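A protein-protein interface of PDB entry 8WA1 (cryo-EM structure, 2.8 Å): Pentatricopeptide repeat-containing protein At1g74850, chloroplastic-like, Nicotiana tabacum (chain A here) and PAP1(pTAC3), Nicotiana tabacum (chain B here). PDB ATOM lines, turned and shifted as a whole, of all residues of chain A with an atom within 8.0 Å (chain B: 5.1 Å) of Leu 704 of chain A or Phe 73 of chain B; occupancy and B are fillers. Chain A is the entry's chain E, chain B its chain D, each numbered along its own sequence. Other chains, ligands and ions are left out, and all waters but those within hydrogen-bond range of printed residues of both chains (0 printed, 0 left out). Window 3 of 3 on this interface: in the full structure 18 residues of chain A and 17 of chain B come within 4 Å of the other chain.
Of the printed residues of chain B, Arg 700 of chain A touches Asp 95 (2.6 Å). Of chain B, only Phe 73 (3.5 Å), Glu 76 (3.3 Å) and Asp 95 (3.4 Å) come within 4 Å of Leu 704 of chain A. Printed residues of chain B within 4 Å of Val 705 of chain A: Asp 95 and Ala 99. Leu 739 of chain A touches none of the printed residues of chain B. Leu 101 of chain B touches none of the printed residues of chain A. The nearest printed residue of chain B that does not touch Arg 700 of chain A is Val 92 of chain B (5.9 Å).
Among the printed residues, pairs that only touch across the chains: Leu 704 of chain A with Glu 76 of chain B, Leu 704 of chain A with Asp 95 of chain B, Leu 704 of chain A with Phe 73 of chain B, Val 705 of chain A with Asp 95 of chain B, Leu 742 of chain A with Ala 99 of chain B, Leu 742 of chain A with Leu 69 of chain B and Val 705 of chain A with Ala 99 of chain B.
NH2 of Arg 700 of chain A lies within salt-bridge range of OD1 of Asp 95 of chain B, at 2.6 Å. OD2 of Asp 95 of chain B lies within hydrogen-bond range of ND2 of Asn 702 of chain A (3.2 Å).
Of the 15 printed residues of chain B, 5 touch a printed residue of chain A. Of the 15 printed residues of chain A, 5 touch a printed residue of chain B. Printed residues of chain A that touch a printed residue of chain B: Arg 700, Asn 702, Leu 704, Val 705 and Leu 742. Hydrophobic or aromatic side chains of chain A within 4 Å of the printed part of chain B: Leu 704, Val 705 and Leu 742.
OE1 of Glu 76 of chain B is in salt-bridge range of NH2 of Arg 80 of chain B, at 3.2 Å. The backbone NH (N) of Ser 707 of chain A sits at hydrogen-bond distance from the backbone carbonyl oxygen (O) of Arg 700 of chain A, 3.2 Å away. The backbone NH (N) of Gln 741 of chain A sits at hydrogen-bond distance from the backbone carbonyl oxygen (O) of Leu 704 of chain A (3.1 Å).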
ATOM      1  N   ARG A 700       1.831   6.115 -29.614  1.00  0.00           N
ATOM      2  CA  ARG A 700       0.853   5.167 -29.100  1.00  0.00           C
ATOM      3  C   ARG A 700      -0.508   5.843 -29.077  1.00  0.00           C
ATOM      4  O   ARG A 700      -0.692   6.849 -28.384  1.00  0.00           O
ATOM      5  CB  ARG A 700       1.228   4.679 -27.693  1.00  0.00           C
ATOM      6  CG  ARG A 700       2.302   3.608 -27.665  1.00  0.00           C
ATOM      7  CD  ARG A 700       1.790   2.286 -28.220  1.00  0.00           C
ATOM      8  NE  ARG A 700       0.645   1.775 -27.468  1.00  0.00           N
ATOM      9  CZ  ARG A 700      -0.614   1.824 -27.893  1.00  0.00           C
ATOM     10  NH1 ARG A 700      -0.897   2.355 -29.075  1.00  0.00           N
ATOM     11  NH2 ARG A 700      -1.590   1.336 -27.139  1.00  0.00           N
ATOM     12  N   ARG A 701      -1.461   5.284 -29.820  1.00  0.00           N
ATOM     13  CA  ARG A 701      -2.793   5.859 -29.955  1.00  0.00           C
ATOM     14  C   ARG A 701      -3.828   4.860 -29.465  1.00  0.00           C
ATOM     15  O   ARG A 701      -3.874   3.721 -29.940  1.00  0.00           O
ATOM     16  CB  ARG A 701      -3.078   6.256 -31.410  1.00  0.00           C
ATOM     17  CG  ARG A 701      -4.559   6.369 -31.763  1.00  0.00           C
ATOM     18  CD  ARG A 701      -5.267   7.461 -30.968  1.00  0.00           C
ATOM     19  NE  ARG A 701      -4.892   8.803 -31.401  1.00  0.00           N
ATOM     20  CZ  ARG A 701      -5.434   9.918 -30.918  1.00  0.00           C
ATOM     21  NH1 ARG A 701      -6.376   9.849 -29.986  1.00  0.00           N
ATOM     22  NH2 ARG A 701      -5.039  11.099 -31.369  1.00  0.00           N
ATOM     23  N   ASN A 702      -4.655   5.293 -28.518  1.00  0.00           N
ATOM     24  CA  ASN A 702      -5.751   4.483 -28.006  1.00  0.00           C
ATOM     25  C   ASN A 702      -6.761   5.418 -27.355  1.00  0.00           C
ATOM     26  O   ASN A 702      -6.487   6.599 -27.129  1.00  0.00           O
ATOM     27  CB  ASN A 702      -5.252   3.419 -27.020  1.00  0.00           C
ATOM     28  CG  ASN A 702      -6.206   2.246 -26.897  1.00  0.00           C
ATOM     29  OD1 ASN A 702      -7.416   2.392 -27.070  1.00  0.00           O
ATOM     30  ND2 ASN A 702      -5.662   1.072 -26.595  1.00  0.00           N
ATOM     31  N   LYS A 703      -7.946   4.873 -27.071  1.00  0.00           N
ATOM     32  CA  LYS A 703      -9.009   5.680 -26.479  1.00  0.00           C
ATOM     33  C   LYS A 703      -8.602   6.219 -25.113  1.00  0.00           C
ATOM     34  O   LYS A 703      -8.833   7.394 -24.801  1.00  0.00           O
ATOM     35  CB  LYS A 703     -10.291   4.854 -26.372  1.00  0.00           C
ATOM     36  CG  LYS A 703     -11.430   5.575 -25.674  1.00  0.00           C
ATOM     37  CD  LYS A 703     -11.836   6.828 -26.432  1.00  0.00           C
ATOM     38  CE  LYS A 703     -12.896   7.604 -25.671  1.00  0.00           C
ATOM     39  NZ  LYS A 703     -14.090   6.765 -25.378  1.00  0.00           N
ATOM     40  N   LEU A 704      -7.980   5.375 -24.289  1.00  0.00           N
ATOM     41  CA  LEU A 704      -7.672   5.770 -22.917  1.00  0.00           C
ATOM     42  C   LEU A 704      -6.522   6.771 -22.870  1.00  0.00           C
ATOM     43  O   LEU A 704      -6.591   7.775 -22.151  1.00  0.00           O
ATOM     44  CB  LEU A 704      -7.362   4.535 -22.065  1.00  0.00           C
ATOM     45  CG  LEU A 704      -6.240   3.564 -22.448  1.00  0.00           C
ATOM     46  CD1 LEU A 704      -5.800   2.776 -21.230  1.00  0.00           C
ATOM     47  CD2 LEU A 704      -6.676   2.607 -23.542  1.00  0.00           C
ATOM     48  N   VAL A 705      -5.457   6.519 -23.625  1.00  0.00           N
ATOM     49  CA  VAL A 705      -4.259   7.349 -23.570  1.00  0.00           C
ATOM     50  C   VAL A 705      -3.746   7.596 -24.982  1.00  0.00           C
ATOM     51  O   VAL A 705      -3.874   6.740 -25.864  1.00  0.00           O
ATOM     52  CB  VAL A 705      -3.165   6.703 -22.691  1.00  0.00           C
ATOM     53  CG1 VAL A 705      -2.596   5.468 -23.362  1.00  0.00           C
ATOM     54  CG2 VAL A 705      -2.061   7.704 -22.373  1.00  0.00           C
ATOM     55  N   TRP A 706      -3.188   8.785 -25.196  1.00  0.00           N
ATOM     56  CA  TRP A 706      -2.451   9.125 -26.407  1.00  0.00           C
ATOM     57  C   TRP A 706      -1.153   9.794 -25.981  1.00  0.00           C
ATOM     58  O   TRP A 706      -1.172  10.917 -25.465  1.00  0.00           O
ATOM     59  CB  TRP A 706      -3.265  10.050 -27.314  1.00  0.00           C
ATOM     60  CG  TRP A 706      -2.644  10.271 -28.656  1.00  0.00           C
ATOM     61  CD1 TRP A 706      -1.930   9.369 -29.388  1.00  0.00           C
ATOM     62  CD2 TRP A 706      -2.669  11.480 -29.422  1.00  0.00           C
ATOM     63  NE1 TRP A 706      -1.517   9.938 -30.568  1.00  0.00           N
ATOM     64  CE2 TRP A 706      -1.959  11.234 -30.613  1.00  0.00           C
ATOM     65  CE3 TRP A 706      -3.230  12.745 -29.219  1.00  0.00           C
ATOM     66  CZ2 TRP A 706      -1.790  12.207 -31.596  1.00  0.00           C
ATOM     67  CZ3 TRP A 706      -3.063  13.707 -30.196  1.00  0.00           C
ATOM     68  CH2 TRP A 706      -2.349  13.434 -31.369  1.00  0.00           C
ATOM     69  N   SER A 707      -0.030   9.110 -26.191  1.00  0.00           N
ATOM     70  CA  SER A 707       1.243   9.565 -25.657  1.00  0.00           C
ATOM     71  C   SER A 707       2.335   9.451 -26.711  1.00  0.00           C
ATOM     72  O   SER A 707       2.229   8.683 -27.672  1.00  0.00           O
ATOM     73  CB  SER A 707       1.644   8.771 -24.407  1.00  0.00           C
ATOM     74  OG  SER A 707       2.943   9.134 -23.971  1.00  0.00           O
ATOM     75  N   GLU A 738     -12.996  11.740 -30.042  1.00  0.00           N
ATOM     76  CA  GLU A 738     -12.887  11.697 -28.591  1.00  0.00           C
ATOM     77  C   GLU A 738     -11.451  11.952 -28.155  1.00  0.00           C
ATOM     78  O   GLU A 738     -10.505  11.405 -28.732  1.00  0.00           O
ATOM     79  CB  GLU A 738     -13.365  10.344 -28.061  1.00  0.00           C
ATOM     80  CG  GLU A 738     -14.803   9.994 -28.412  1.00  0.00           C
ATOM     81  CD  GLU A 738     -14.944   9.408 -29.804  1.00  0.00           C
ATOM     82  OE1 GLU A 738     -13.907   9.089 -30.423  1.00  0.00           O
ATOM     83  OE2 GLU A 738     -16.090   9.270 -30.281  1.00  0.00           O
ATOM     84  N   LEU A 739     -11.289  12.784 -27.130  1.00  0.00           N
ATOM     85  CA  LEU A 739      -9.969  13.119 -26.616  1.00  0.00           C
ATOM     86  C   LEU A 739      -9.522  12.054 -25.621  1.00  0.00           C
ATOM     87  O   LEU A 739     -10.363  11.421 -24.971  1.00  0.00           O
ATOM     88  CB  LEU A 739      -9.985  14.501 -25.956  1.00  0.00           C
ATOM     89  CG  LEU A 739     -10.530  15.654 -26.801  1.00  0.00           C
ATOM     90  CD1 LEU A 739     -10.581  16.942 -25.990  1.00  0.00           C
ATOM     91  CD2 LEU A 739      -9.699  15.842 -28.060  1.00  0.00           C
ATOM     92  N   PRO A 740      -8.218  11.829 -25.470  1.00  0.00           N
ATOM     93  CA  PRO A 740      -7.757  10.844 -24.488  1.00  0.00           C
ATOM     94  C   PRO A 740      -7.896  11.367 -23.069  1.00  0.00           C
ATOM     95  O   PRO A 740      -7.796  12.570 -22.811  1.00  0.00           O
ATOM     96  CB  PRO A 740      -6.287  10.631 -24.863  1.00  0.00           C
ATOM     97  CG  PRO A 740      -5.886  11.904 -25.528  1.00  0.00           C
ATOM     98  CD  PRO A 740      -7.108  12.391 -26.258  1.00  0.00           C
ATOM     99  N   GLN A 741      -8.139  10.437 -22.143  1.00  0.00           N
ATOM    100  CA  GLN A 741      -8.284  10.809 -20.739  1.00  0.00           C
ATOM    101  C   GLN A 741      -7.015  11.465 -20.209  1.00  0.00           C
ATOM    102  O   GLN A 741      -7.079  12.364 -19.362  1.00  0.00           O
ATOM    103  CB  GLN A 741      -8.649   9.582 -19.902  1.00  0.00           C
ATOM    104  CG  GLN A 741     -10.119   9.174 -19.981  1.00  0.00           C
ATOM    105  CD  GLN A 741     -10.525   8.661 -21.351  1.00  0.00           C
ATOM    106  OE1 GLN A 741      -9.680   8.277 -22.160  1.00  0.00           O
ATOM    107  NE2 GLN A 741     -11.826   8.654 -21.618  1.00  0.00           N
ATOM    108  N   LEU A 742      -5.855  11.030 -20.694  1.00  0.00           N
ATOM    109  CA  LEU A 742      -4.579  11.620 -20.316  1.00  0.00           C
ATOM    110  C   LEU A 742      -3.673  11.677 -21.537  1.00  0.00           C
ATOM    111  O   LEU A 742      -3.390  10.643 -22.150  1.00  0.00           O
ATOM    112  CB  LEU A 742      -3.907  10.821 -19.194  1.00  0.00           C
ATOM    113  CG  LEU A 742      -2.747  11.514 -18.480  1.00  0.00           C
ATOM    114  CD1 LEU A 742      -3.252  12.710 -17.688  1.00  0.00           C
ATOM    115  CD2 LEU A 742      -2.005  10.539 -17.577  1.00  0.00           C
ATOM    116  N   ALA A 743      -3.225  12.879 -21.886  1.00  0.00           N
ATOM    117  CA  ALA A 743      -2.271  13.081 -22.968  1.00  0.00           C
ATOM    118  C   ALA A 743      -0.891  13.291 -22.359  1.00  0.00           C
ATOM    119  O   ALA A 743      -0.642  14.317 -21.718  1.00  0.00           O
ATOM    120  CB  ALA A 743      -2.668  14.273 -23.837  1.00  0.00           C
ATOM    121  N   LYS A 793      -7.797  15.752 -20.196  1.00  0.00           N
ATOM    122  CA  LYS A 793      -8.686  15.899 -21.345  1.00  0.00           C
ATOM    123  C   LYS A 793      -9.314  17.286 -21.385  1.00  0.00           C
ATOM    124  O   LYS A 793      -9.374  17.917 -22.448  1.00  0.00           O
ATOM    125  CB  LYS A 793      -9.762  14.813 -21.314  1.00  0.00           C
ATOM    126  CG  LYS A 793     -10.346  14.549 -19.937  1.00  0.00           C
ATOM    127  CD  LYS A 793     -11.305  13.370 -19.959  1.00  0.00           C
ATOM    128  CE  LYS A 793     -11.778  13.018 -18.557  1.00  0.00           C
ATOM    129  NZ  LYS A 793     -12.709  11.855 -18.558  1.00  0.00           N
ATOM    130  N   LEU B  69      -8.093   8.050 -13.119  1.00  0.00           N
ATOM    131  CA  LEU B  69      -7.431   7.448 -14.272  1.00  0.00           C
ATOM    132  C   LEU B  69      -7.363   5.931 -14.144  1.00  0.00           C
ATOM    133  O   LEU B  69      -7.589   5.207 -15.123  1.00  0.00           O
ATOM    134  CB  LEU B  69      -6.029   8.031 -14.439  1.00  0.00           C
ATOM    135  CG  LEU B  69      -5.945   9.532 -14.710  1.00  0.00           C
ATOM    136  CD1 LEU B  69      -4.497   9.953 -14.872  1.00  0.00           C
ATOM    137  CD2 LEU B  69      -6.757   9.902 -15.939  1.00  0.00           C
ATOM    138  N   ARG B  70      -7.044   5.433 -12.944  1.00  0.00           N
ATOM    139  CA  ARG B  70      -6.946   3.995 -12.743  1.00  0.00           C
ATOM    140  C   ARG B  70      -8.286   3.312 -12.966  1.00  0.00           C
ATOM    141  O   ARG B  70      -8.325   2.177 -13.448  1.00  0.00           O
ATOM    142  CB  ARG B  70      -6.419   3.693 -11.339  1.00  0.00           C
ATOM    143  CG  ARG B  70      -5.305   2.656 -11.304  1.00  0.00           C
ATOM    144  CD  ARG B  70      -3.986   3.244 -11.782  1.00  0.00           C
ATOM    145  NE  ARG B  70      -3.426   4.180 -10.811  1.00  0.00           N
ATOM    146  CZ  ARG B  70      -2.481   3.868  -9.930  1.00  0.00           C
ATOM    147  NH1 ARG B  70      -1.981   2.641  -9.897  1.00  0.00           N
ATOM    148  NH2 ARG B  70      -2.034   4.785  -9.083  1.00  0.00           N
ATOM    149  N   LEU B  71      -9.390   3.988 -12.643  1.00  0.00           N
ATOM    150  CA  LEU B  71     -10.711   3.424 -12.910  1.00  0.00           C
ATOM    151  C   LEU B  71     -10.917   3.193 -14.402  1.00  0.00           C
ATOM    152  O   LEU B  71     -11.281   2.090 -14.827  1.00  0.00           O
ATOM    153  CB  LEU B  71     -11.796   4.345 -12.351  1.00  0.00           C
ATOM    154  CG  LEU B  71     -13.225   4.117 -12.854  1.00  0.00           C
ATOM    155  CD1 LEU B  71     -13.720   2.719 -12.503  1.00  0.00           C
ATOM    156  CD2 LEU B  71     -14.165   5.177 -12.297  1.00  0.00           C
ATOM    157  N   VAL B  72     -10.690   4.230 -15.211  1.00  0.00           N
ATOM    158  CA  VAL B  72     -10.909   4.120 -16.650  1.00  0.00           C
ATOM    159  C   VAL B  72      -9.957   3.099 -17.264  1.00  0.00           C
ATOM    160  O   VAL B  72     -10.330   2.363 -18.187  1.00  0.00           O
ATOM    161  CB  VAL B  72     -10.768   5.502 -17.315  1.00  0.00           C
ATOM    162  CG1 VAL B  72     -11.057   5.412 -18.806  1.00  0.00           C
ATOM    163  CG2 VAL B  72     -11.698   6.506 -16.648  1.00  0.00           C
ATOM    164  N   PHE B  73      -8.721   3.027 -16.762  1.00  0.00           N
ATOM    165  CA  PHE B  73      -7.765   2.075 -17.323  1.00  0.00           C
ATOM    166  C   PHE B  73      -8.129   0.640 -16.950  1.00  0.00           C
ATOM    167  O   PHE B  73      -8.159  -0.247 -17.816  1.00  0.00           O
ATOM    168  CB  PHE B  73      -6.349   2.421 -16.855  1.00  0.00           C
ATOM    169  CG  PHE B  73      -5.707   3.547 -17.627  1.00  0.00           C
ATOM    170  CD1 PHE B  73      -6.392   4.727 -17.869  1.00  0.00           C
ATOM    171  CD2 PHE B  73      -4.411   3.429 -18.096  1.00  0.00           C
ATOM    172  CE1 PHE B  73      -5.799   5.760 -18.572  1.00  0.00           C
ATOM    173  CE2 PHE B  73      -3.812   4.458 -18.800  1.00  0.00           C
ATOM    174  CZ  PHE B  73      -4.508   5.624 -19.037  1.00  0.00           C
ATOM    175  N   MET B  74      -8.421   0.395 -15.670  1.00  0.00           N
ATOM    176  CA  MET B  74      -8.795  -0.934 -15.209  1.00  0.00           C
ATOM    177  C   MET B  74     -10.112  -1.402 -15.808  1.00  0.00           C
ATOM    178  O   MET B  74     -10.312  -2.611 -15.947  1.00  0.00           O
ATOM    179  CB  MET B  74      -8.879  -0.949 -13.682  1.00  0.00           C
ATOM    180  CG  MET B  74      -8.970  -2.336 -13.071  1.00  0.00           C
ATOM    181  SD  MET B  74      -7.428  -3.258 -13.221  1.00  0.00           S
ATOM    182  CE  MET B  74      -6.325  -2.224 -12.261  1.00  0.00           C
ATOM    183  N   GLU B  75     -11.008  -0.482 -16.173  1.00  0.00           N
ATOM    184  CA  GLU B  75     -12.239  -0.886 -16.845  1.00  0.00           C
ATOM    185  C   GLU B  75     -11.930  -1.623 -18.142  1.00  0.00           C
ATOM    186  O   GLU B  75     -12.385  -2.753 -18.355  1.00  0.00           O
ATOM    187  CB  GLU B  75     -13.115   0.341 -17.109  1.00  0.00           C
ATOM    188  CG  GLU B  75     -14.610   0.087 -16.983  1.00  0.00           C
ATOM    189  CD  GLU B  75     -15.156  -0.799 -18.085  1.00  0.00           C
ATOM    190  OE1 GLU B  75     -14.638  -0.730 -19.220  1.00  0.00           O
ATOM    191  OE2 GLU B  75     -16.105  -1.564 -17.817  1.00  0.00           O
ATOM    192  N   GLU B  76     -11.136  -1.000 -19.017  1.00  0.00           N
ATOM    193  CA  GLU B  76     -10.766  -1.648 -20.271  1.00  0.00           C
ATOM    194  C   GLU B  76      -9.887  -2.867 -20.028  1.00  0.00           C
ATOM    195  O   GLU B  76      -9.982  -3.858 -20.761  1.00  0.00           O
ATOM    196  CB  GLU B  76     -10.064  -0.656 -21.196  1.00  0.00           C
ATOM    197  CG  GLU B  76     -10.974   0.429 -21.746  1.00  0.00           C
ATOM    198  CD  GLU B  76     -10.345   1.193 -22.893  1.00  0.00           C
ATOM    199  OE1 GLU B  76      -9.354   0.697 -23.470  1.00  0.00           O
ATOM    200  OE2 GLU B  76     -10.842   2.291 -23.220  1.00  0.00           O
ATOM    201  N   LEU B  77      -9.024  -2.817 -19.009  1.00  0.00           N
ATOM    202  CA  LEU B  77      -8.188  -3.977 -18.707  1.00  0.00           C
ATOM    203  C   LEU B  77      -9.045  -5.193 -18.367  1.00  0.00           C
ATOM    204  O   LEU B  77      -8.865  -6.277 -18.936  1.00  0.00           O
ATOM    205  CB  LEU B  77      -7.224  -3.651 -17.565  1.00  0.00           C
ATOM    206  CG  LEU B  77      -6.157  -4.704 -17.248  1.00  0.00           C
ATOM    207  CD1 LEU B  77      -4.809  -4.044 -17.010  1.00  0.00           C
ATOM    208  CD2 LEU B  77      -6.556  -5.549 -16.044  1.00  0.00           C
ATOM    209  N   ARG B  80     -11.059  -6.435 -21.502  1.00  0.00           N
ATOM    210  CA  ARG B  80     -10.245  -7.241 -22.402  1.00  0.00           C
ATOM    211  C   ARG B  80      -9.892  -8.583 -21.773  1.00  0.00           C
ATOM    212  O   ARG B  80      -9.744  -9.588 -22.478  1.00  0.00           O
ATOM    213  CB  ARG B  80      -8.979  -6.480 -22.793  1.00  0.00           C
ATOM    214  CG  ARG B  80      -8.774  -6.363 -24.294  1.00  0.00           C
ATOM    215  CD  ARG B  80      -9.718  -5.344 -24.908  1.00  0.00           C
ATOM    216  NE  ARG B  80      -9.346  -3.976 -24.556  1.00  0.00           N
ATOM    217  CZ  ARG B  80      -8.506  -3.228 -25.263  1.00  0.00           C
ATOM    218  NH1 ARG B  80      -7.948  -3.713 -26.363  1.00  0.00           N
ATOM    219  NH2 ARG B  80      -8.221  -1.994 -24.871  1.00  0.00           N
ATOM    220  N   VAL B  92      -3.131  -2.507 -22.917  1.00  0.00           N
ATOM    221  CA  VAL B  92      -3.579  -1.688 -21.792  1.00  0.00           C
ATOM    222  C   VAL B  92      -2.475  -1.557 -20.749  1.00  0.00           C
ATOM    223  O   VAL B  92      -2.293  -0.492 -20.147  1.00  0.00           O
ATOM    224  CB  VAL B  92      -4.871  -2.273 -21.188  1.00  0.00           C
ATOM    225  CG1 VAL B  92      -5.223  -1.571 -19.885  1.00  0.00           C
ATOM    226  CG2 VAL B  92      -6.020  -2.152 -22.177  1.00  0.00           C
ATOM    227  N   ASP B  95      -0.083   0.873 -22.022  1.00  0.00           N
ATOM    228  CA  ASP B  95      -0.696   2.195 -21.938  1.00  0.00           C
ATOM    229  C   ASP B  95      -0.593   2.757 -20.527  1.00  0.00           C
ATOM    230  O   ASP B  95      -0.330   3.951 -20.344  1.00  0.00           O
ATOM    231  CB  ASP B  95      -2.154   2.123 -22.385  1.00  0.00           C
ATOM    232  CG  ASP B  95      -2.294   1.904 -23.877  1.00  0.00           C
ATOM    233  OD1 ASP B  95      -1.256   1.800 -24.562  1.00  0.00           O
ATOM    234  OD2 ASP B  95      -3.441   1.834 -24.366  1.00  0.00           O
ATOM    235  N   MET B  96      -0.807   1.911 -19.517  1.00  0.00           N
ATOM    236  CA  MET B  96      -0.603   2.343 -18.136  1.00  0.00           C
ATOM    237  C   MET B  96       0.852   2.719 -17.894  1.00  0.00           C
ATOM    238  O   MET B  96       1.142   3.704 -17.205  1.00  0.00           O
ATOM    239  CB  MET B  96      -1.030   1.245 -17.161  1.00  0.00           C
ATOM    240  CG  MET B  96      -2.471   0.796 -17.293  1.00  0.00           C
ATOM    241  SD  MET B  96      -3.018  -0.156 -15.865  1.00  0.00           S
ATOM    242  CE  MET B  96      -1.636  -1.276 -15.668  1.00  0.00           C
ATOM    243  N   ALA B  99       1.429   6.128 -19.640  1.00  0.00           N
ATOM    244  CA  ALA B  99       0.714   7.208 -18.973  1.00  0.00           C
ATOM    245  C   ALA B  99       1.211   7.462 -17.556  1.00  0.00           C
ATOM    246  O   ALA B  99       0.741   8.407 -16.914  1.00  0.00           O
ATOM    247  CB  ALA B  99      -0.786   6.908 -18.947  1.00  0.00           C
ATOM    248  N   LEU B 101       0.883   5.393 -14.915  1.00  0.00           N
ATOM    249  CA  LEU B 101       0.192   4.581 -13.918  1.00  0.00           C
ATOM    250  C   LEU B 101       0.922   3.250 -13.788  1.00  0.00           C
ATOM    251  O   LEU B 101       0.780   2.368 -14.641  1.00  0.00           O
ATOM    252  CB  LEU B 101      -1.266   4.374 -14.315  1.00  0.00           C
ATOM    253  CG  LEU B 101      -2.095   5.636 -14.560  1.00  0.00           C
ATOM    254  CD1 LEU B 101      -3.493   5.276 -15.042  1.00  0.00           C
ATOM    255  CD2 LEU B 101      -2.163   6.494 -13.306  1.00  0.00           C
